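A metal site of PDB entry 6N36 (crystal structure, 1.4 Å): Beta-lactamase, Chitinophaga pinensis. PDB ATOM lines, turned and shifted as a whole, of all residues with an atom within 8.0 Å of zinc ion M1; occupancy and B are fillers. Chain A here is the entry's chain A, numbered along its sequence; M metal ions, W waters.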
ATOM      1  N   TRP A  16     -32.953  13.599   8.637  1.00  0.00           N
ATOM      2  CA  TRP A  16     -33.718  14.417   9.626  1.00  0.00           C
ATOM      3  C   TRP A  16     -35.224  14.289   9.372  1.00  0.00           C
ATOM      4  O   TRP A  16     -36.014  14.399  10.322  1.00  0.00           O
ATOM      5  CB  TRP A  16     -33.313  15.895   9.560  1.00  0.00           C
ATOM      6  CG  TRP A  16     -31.965  16.177  10.127  1.00  0.00           C
ATOM      7  CD1 TRP A  16     -31.060  15.289  10.619  1.00  0.00           C
ATOM      8  CD2 TRP A  16     -31.346  17.468  10.168  1.00  0.00           C
ATOM      9  NE1 TRP A  16     -29.910  15.953  10.974  1.00  0.00           N
ATOM     10  CE2 TRP A  16     -30.084  17.291  10.758  1.00  0.00           C
ATOM     11  CE3 TRP A  16     -31.750  18.751   9.754  1.00  0.00           C
ATOM     12  CZ2 TRP A  16     -29.203  18.374  10.907  1.00  0.00           C
ATOM     13  CZ3 TRP A  16     -30.897  19.816   9.942  1.00  0.00           C
ATOM     14  CH2 TRP A  16     -29.627  19.608  10.488  1.00  0.00           C
ATOM     15  N   ASP A  36     -33.169  10.178  12.105  1.00  0.00           N
ATOM     16  CA  ASP A  36     -32.015  10.771  12.800  1.00  0.00           C
ATOM     17  C   ASP A  36     -32.468  11.570  14.010  1.00  0.00           C
ATOM     18  O   ASP A  36     -31.677  11.652  15.001  1.00  0.00           O
ATOM     19  CB  ASP A  36     -31.148  11.630  11.880  1.00  0.00           C
ATOM     20  CG  ASP A  36     -29.869  12.014  12.580  1.00  0.00           C
ATOM     21  OD1 ASP A  36     -29.136  11.071  13.005  1.00  0.00           O
ATOM     22  OD2 ASP A  36     -29.626  13.220  12.732  1.00  0.00           O
ATOM     23  N   LEU A  37     -33.574  12.289  13.940  1.00  0.00           N
ATOM     24  CA  LEU A  37     -33.878  13.294  15.013  1.00  0.00           C
ATOM     25  C   LEU A  37     -34.749  12.676  16.098  1.00  0.00           C
ATOM     26  O   LEU A  37     -35.902  12.267  15.873  1.00  0.00           O
ATOM     27  CB  LEU A  37     -34.554  14.521  14.426  1.00  0.00           C
ATOM     28  CG  LEU A  37     -33.744  15.339  13.449  1.00  0.00           C
ATOM     29  CD1 LEU A  37     -34.533  16.520  12.985  1.00  0.00           C
ATOM     30  CD2 LEU A  37     -32.416  15.765  14.072  1.00  0.00           C
ATOM     31  N   ASN A  52     -38.399  17.729  22.321  1.00  0.00           N
ATOM     32  CA  ASN A  52     -37.924  18.084  20.970  1.00  0.00           C
ATOM     33  C   ASN A  52     -38.983  17.910  19.899  1.00  0.00           C
ATOM     34  O   ASN A  52     -39.866  17.024  19.977  1.00  0.00           O
ATOM     35  CB  ASN A  52     -36.685  17.325  20.523  1.00  0.00           C
ATOM     36  CG  ASN A  52     -35.436  17.692  21.302  1.00  0.00           C
ATOM     37  OD1 ASN A  52     -35.378  18.763  21.938  1.00  0.00           O
ATOM     38  ND2 ASN A  52     -34.446  16.801  21.291  1.00  0.00           N
ATOM     39  N   THR A  82     -33.925  19.803  24.205  1.00  0.00           N
ATOM     40  CA  THR A  82     -32.520  19.633  24.606  1.00  0.00           C
ATOM     41  C   THR A  82     -31.658  20.849  24.256  1.00  0.00           C
ATOM     42  O   THR A  82     -30.684  21.133  24.973  1.00  0.00           O
ATOM     43  CB  THR A  82     -31.939  18.344  24.066  1.00  0.00           C
ATOM     44  OG1 THR A  82     -32.042  18.296  22.645  1.00  0.00           O
ATOM     45  CG2 THR A  82     -32.602  17.123  24.673  1.00  0.00           C
ATOM     46  N   HIS A  83     -31.907  21.530  23.171  1.00  0.00           N
ATOM     47  CA  HIS A  83     -31.229  22.819  22.856  1.00  0.00           C
ATOM     48  C   HIS A  83     -31.964  23.522  21.738  1.00  0.00           C
ATOM     49  O   HIS A  83     -32.482  22.843  20.834  1.00  0.00           O
ATOM     50  CB  HIS A  83     -29.741  22.626  22.522  1.00  0.00           C
ATOM     51  CG  HIS A  83     -29.401  21.920  21.244  1.00  0.00           C
ATOM     52  ND1 HIS A  83     -29.125  20.582  21.162  1.00  0.00           N
ATOM     53  CD2 HIS A  83     -29.161  22.412  20.019  1.00  0.00           C
ATOM     54  CE1 HIS A  83     -28.739  20.284  19.928  1.00  0.00           C
ATOM     55  NE2 HIS A  83     -28.741  21.384  19.203  1.00  0.00           N
ATOM     56  N   HIS A  85     -31.679  24.777  18.692  1.00  0.00           N
ATOM     57  CA  HIS A  85     -31.318  24.797  17.262  1.00  0.00           C
ATOM     58  C   HIS A  85     -32.515  24.356  16.436  1.00  0.00           C
ATOM     59  O   HIS A  85     -33.345  23.558  16.913  1.00  0.00           O
ATOM     60  CB  HIS A  85     -30.099  23.902  16.976  1.00  0.00           C
ATOM     61  CG  HIS A  85     -28.769  24.493  17.328  1.00  0.00           C
ATOM     62  ND1 HIS A  85     -27.608  23.726  17.489  1.00  0.00           N
ATOM     63  CD2 HIS A  85     -28.418  25.772  17.588  1.00  0.00           C
ATOM     64  CE1 HIS A  85     -26.609  24.532  17.766  1.00  0.00           C
ATOM     65  NE2 HIS A  85     -27.068  25.786  17.820  1.00  0.00           N
ATOM     66  N   TYR A  86     -32.572  24.792  15.185  1.00  0.00           N
ATOM     67  CA  TYR A  86     -33.760  24.600  14.335  1.00  0.00           C
ATOM     68  C   TYR A  86     -34.088  23.117  14.075  1.00  0.00           C
ATOM     69  O   TYR A  86     -35.243  22.844  13.679  1.00  0.00           O
ATOM     70  CB  TYR A  86     -33.613  25.380  13.030  1.00  0.00           C
ATOM     71  CG  TYR A  86     -32.657  24.780  12.033  1.00  0.00           C
ATOM     72  CD1 TYR A  86     -31.305  25.063  12.090  1.00  0.00           C
ATOM     73  CD2 TYR A  86     -33.116  24.003  10.984  1.00  0.00           C
ATOM     74  CE1 TYR A  86     -30.410  24.581  11.139  1.00  0.00           C
ATOM     75  CE2 TYR A  86     -32.256  23.535  10.000  1.00  0.00           C
ATOM     76  CZ  TYR A  86     -30.897  23.832  10.075  1.00  0.00           C
ATOM     77  OH  TYR A  86     -30.030  23.365   9.152  1.00  0.00           O
ATOM     78  N   ASP A  87     -33.147  22.204  14.167  1.00  0.00           N
ATOM     79  CA  ASP A  87     -33.413  20.752  13.977  1.00  0.00           C
ATOM     80  C   ASP A  87     -34.085  20.131  15.205  1.00  0.00           C
ATOM     81  O   ASP A  87     -34.562  18.979  15.117  1.00  0.00           O
ATOM     82  CB  ASP A  87     -32.150  19.998  13.559  1.00  0.00           C
ATOM     83  CG  ASP A  87     -30.978  20.106  14.505  1.00  0.00           C
ATOM     84  OD1 ASP A  87     -30.872  21.184  15.187  1.00  0.00           O
ATOM     85  OD2 ASP A  87     -30.131  19.144  14.512  1.00  0.00           O
ATOM     86  N   HIS A  88     -34.178  20.828  16.354  1.00  0.00           N
ATOM     87  CA  HIS A  88     -34.830  20.329  17.579  1.00  0.00           C
ATOM     88  C   HIS A  88     -36.017  21.184  18.007  1.00  0.00           C
ATOM     89  O   HIS A  88     -36.793  20.696  18.875  1.00  0.00           O
ATOM     90  CB  HIS A  88     -33.824  20.177  18.729  1.00  0.00           C
ATOM     91  CG  HIS A  88     -32.644  19.378  18.266  1.00  0.00           C
ATOM     92  ND1 HIS A  88     -32.730  18.036  17.942  1.00  0.00           N
ATOM     93  CD2 HIS A  88     -31.388  19.790  17.965  1.00  0.00           C
ATOM     94  CE1 HIS A  88     -31.524  17.662  17.458  1.00  0.00           C
ATOM     95  NE2 HIS A  88     -30.689  18.734  17.510  1.00  0.00           N
ATOM     96  N   HIS A 160     -22.936  23.648  23.483  1.00  0.00           N
ATOM     97  CA  HIS A 160     -23.518  23.481  22.117  1.00  0.00           C
ATOM     98  C   HIS A 160     -24.522  24.621  21.856  1.00  0.00           C
ATOM     99  O   HIS A 160     -24.489  25.244  20.798  1.00  0.00           O
ATOM    100  CB  HIS A 160     -24.146  22.098  22.039  1.00  0.00           C
ATOM    101  CG  HIS A 160     -24.630  21.806  20.688  1.00  0.00           C
ATOM    102  ND1 HIS A 160     -23.806  21.304  19.715  1.00  0.00           N
ATOM    103  CD2 HIS A 160     -25.834  22.004  20.130  1.00  0.00           C
ATOM    104  CE1 HIS A 160     -24.497  21.225  18.593  1.00  0.00           C
ATOM    105  NE2 HIS A 160     -25.722  21.640  18.808  1.00  0.00           N
ATOM    106  N   ASN A 184     -27.943  15.668  26.065  1.00  0.00           N
ATOM    107  CA  ASN A 184     -27.486  16.573  24.996  1.00  0.00           C
ATOM    108  C   ASN A 184     -25.968  16.481  24.892  1.00  0.00           C
ATOM    109  O   ASN A 184     -25.264  16.988  25.694  1.00  0.00           O
ATOM    110  CB  ASN A 184     -27.966  18.002  25.202  1.00  0.00           C
ATOM    111  CG  ASN A 184     -27.897  18.732  23.885  1.00  0.00           C
ATOM    112  OD1 ASN A 184     -28.846  18.639  23.075  1.00  0.00           O
ATOM    113  ND2 ASN A 184     -26.778  19.439  23.630  1.00  0.00           N
ATOM    114  N   SER A 187     -21.324  18.300  21.441  1.00  0.00           N
ATOM    115  CA  SER A 187     -20.658  18.479  20.145  1.00  0.00           C
ATOM    116  C   SER A 187     -20.252  19.935  19.929  1.00  0.00           C
ATOM    117  O   SER A 187     -20.941  20.837  20.352  1.00  0.00           O
ATOM    118  CB  SER A 187     -21.484  17.918  19.024  1.00  0.00           C
ATOM    119  OG  SER A 187     -22.692  18.620  18.914  1.00  0.00           O
ATOM    120  N   LEU A 189     -19.135  22.792  17.065  1.00  0.00           N
ATOM    121  CA  LEU A 189     -19.228  23.105  15.621  1.00  0.00           C
ATOM    122  C   LEU A 189     -17.856  23.617  15.171  1.00  0.00           C
ATOM    123  O   LEU A 189     -17.015  24.099  15.990  1.00  0.00           O
ATOM    124  CB  LEU A 189     -20.308  24.147  15.360  1.00  0.00           C
ATOM    125  CG  LEU A 189     -21.737  23.665  15.619  1.00  0.00           C
ATOM    126  CD1 LEU A 189     -22.740  24.748  15.218  1.00  0.00           C
ATOM    127  CD2 LEU A 189     -22.010  22.394  14.875  1.00  0.00           C
ATOM    128  N   PRO A 225     -30.279  13.393  21.035  1.00  0.00           N
ATOM    129  CA  PRO A 225     -31.087  14.036  20.011  1.00  0.00           C
ATOM    130  C   PRO A 225     -30.801  13.573  18.589  1.00  0.00           C
ATOM    131  O   PRO A 225     -31.631  13.845  17.767  1.00  0.00           O
ATOM    132  CB  PRO A 225     -30.750  15.517  20.166  1.00  0.00           C
ATOM    133  CG  PRO A 225     -30.318  15.666  21.589  1.00  0.00           C
ATOM    134  CD  PRO A 225     -29.548  14.389  21.861  1.00  0.00           C
ATOM    135  N   HIS A 226     -29.622  12.991  18.338  1.00  0.00           N
ATOM    136  CA  HIS A 226     -29.267  12.484  17.006  1.00  0.00           C
ATOM    137  C   HIS A 226     -28.982  10.991  17.130  1.00  0.00           C
ATOM    138  O   HIS A 226     -28.185  10.599  17.976  1.00  0.00           O
ATOM    139  CB  HIS A 226     -28.060  13.221  16.436  1.00  0.00           C
ATOM    140  CG  HIS A 226     -28.383  14.611  16.019  1.00  0.00           C
ATOM    141  ND1 HIS A 226     -28.966  14.920  14.776  1.00  0.00           N
ATOM    142  CD2 HIS A 226     -28.266  15.780  16.698  1.00  0.00           C
ATOM    143  CE1 HIS A 226     -29.138  16.230  14.713  1.00  0.00           C
ATOM    144  NE2 HIS A 226     -28.735  16.786  15.854  1.00  0.00           N
ATOM    145  N   GLN A 229     -25.351   9.653  17.610  1.00  0.00           N
ATOM    146  CA  GLN A 229     -24.669   9.962  18.890  1.00  0.00           C
ATOM    147  C   GLN A 229     -24.767   8.761  19.836  1.00  0.00           C
ATOM    148  O   GLN A 229     -23.874   8.625  20.669  1.00  0.00           O
ATOM    149  CB  GLN A 229     -25.251  11.224  19.501  1.00  0.00           C
ATOM    150  CG  GLN A 229     -24.779  12.414  18.697  1.00  0.00           C
ATOM    151  CD  GLN A 229     -25.366  13.715  19.142  1.00  0.00           C
ATOM    152  OE1 GLN A 229     -26.478  13.761  19.664  1.00  0.00           O
ATOM    153  NE2 GLN A 229     -24.592  14.765  18.831  1.00  0.00           N
HETATM  154 ZN    ZN M   1     -28.984  18.804  16.252  1.00  0.00          ZN
HETATM  155 ZN    ZN M   2     -27.385  21.639  17.495  1.00  0.00          ZN
HETATM  156  O   HOH W   1     -28.553  21.374  15.854  1.00  0.00           O
HETATM  157  O   HOH W   2     -27.381  19.221  17.407  1.00  0.00           O
HETATM  158  O   HOH W   3     -25.965  18.730  15.519  1.00  0.00           O
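The backbone NH of His 226 is in hydrogen-bond range of the side-chain amide oxygen of Gln 229 (3.5 Å). OD2 of Asp 36 sits at hydrogen-bond distance from ND1 of His 226 (2.7 Å). OD1 of Asn 184 sits at hydrogen-bond distance from ND1 of His 83, 2.7 Å away.
Zinc ion M1 is bound by water W2 (2.0 Å), a ring nitrogen (NE2) of His 226 (2.1 Å), the side-chain carboxylate of Asp 87 (2.1 Å) and a ring nitrogen (NE2) of His 88 (2.1 Å). Zinc ion M1 has four donor atoms within binding distance. Slightly farther from zinc ion M1 lies water W1 (2.6 Å).
Merely in contact with zinc ion M1: His 83 (3.9 Å). Four residues have an atom within 4 Å of zinc ion M1: His 83, Asp 87, His 88 and His 226. The nearest printed residue that does not touch zinc ion M1 is His 160 (5.0 Å).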
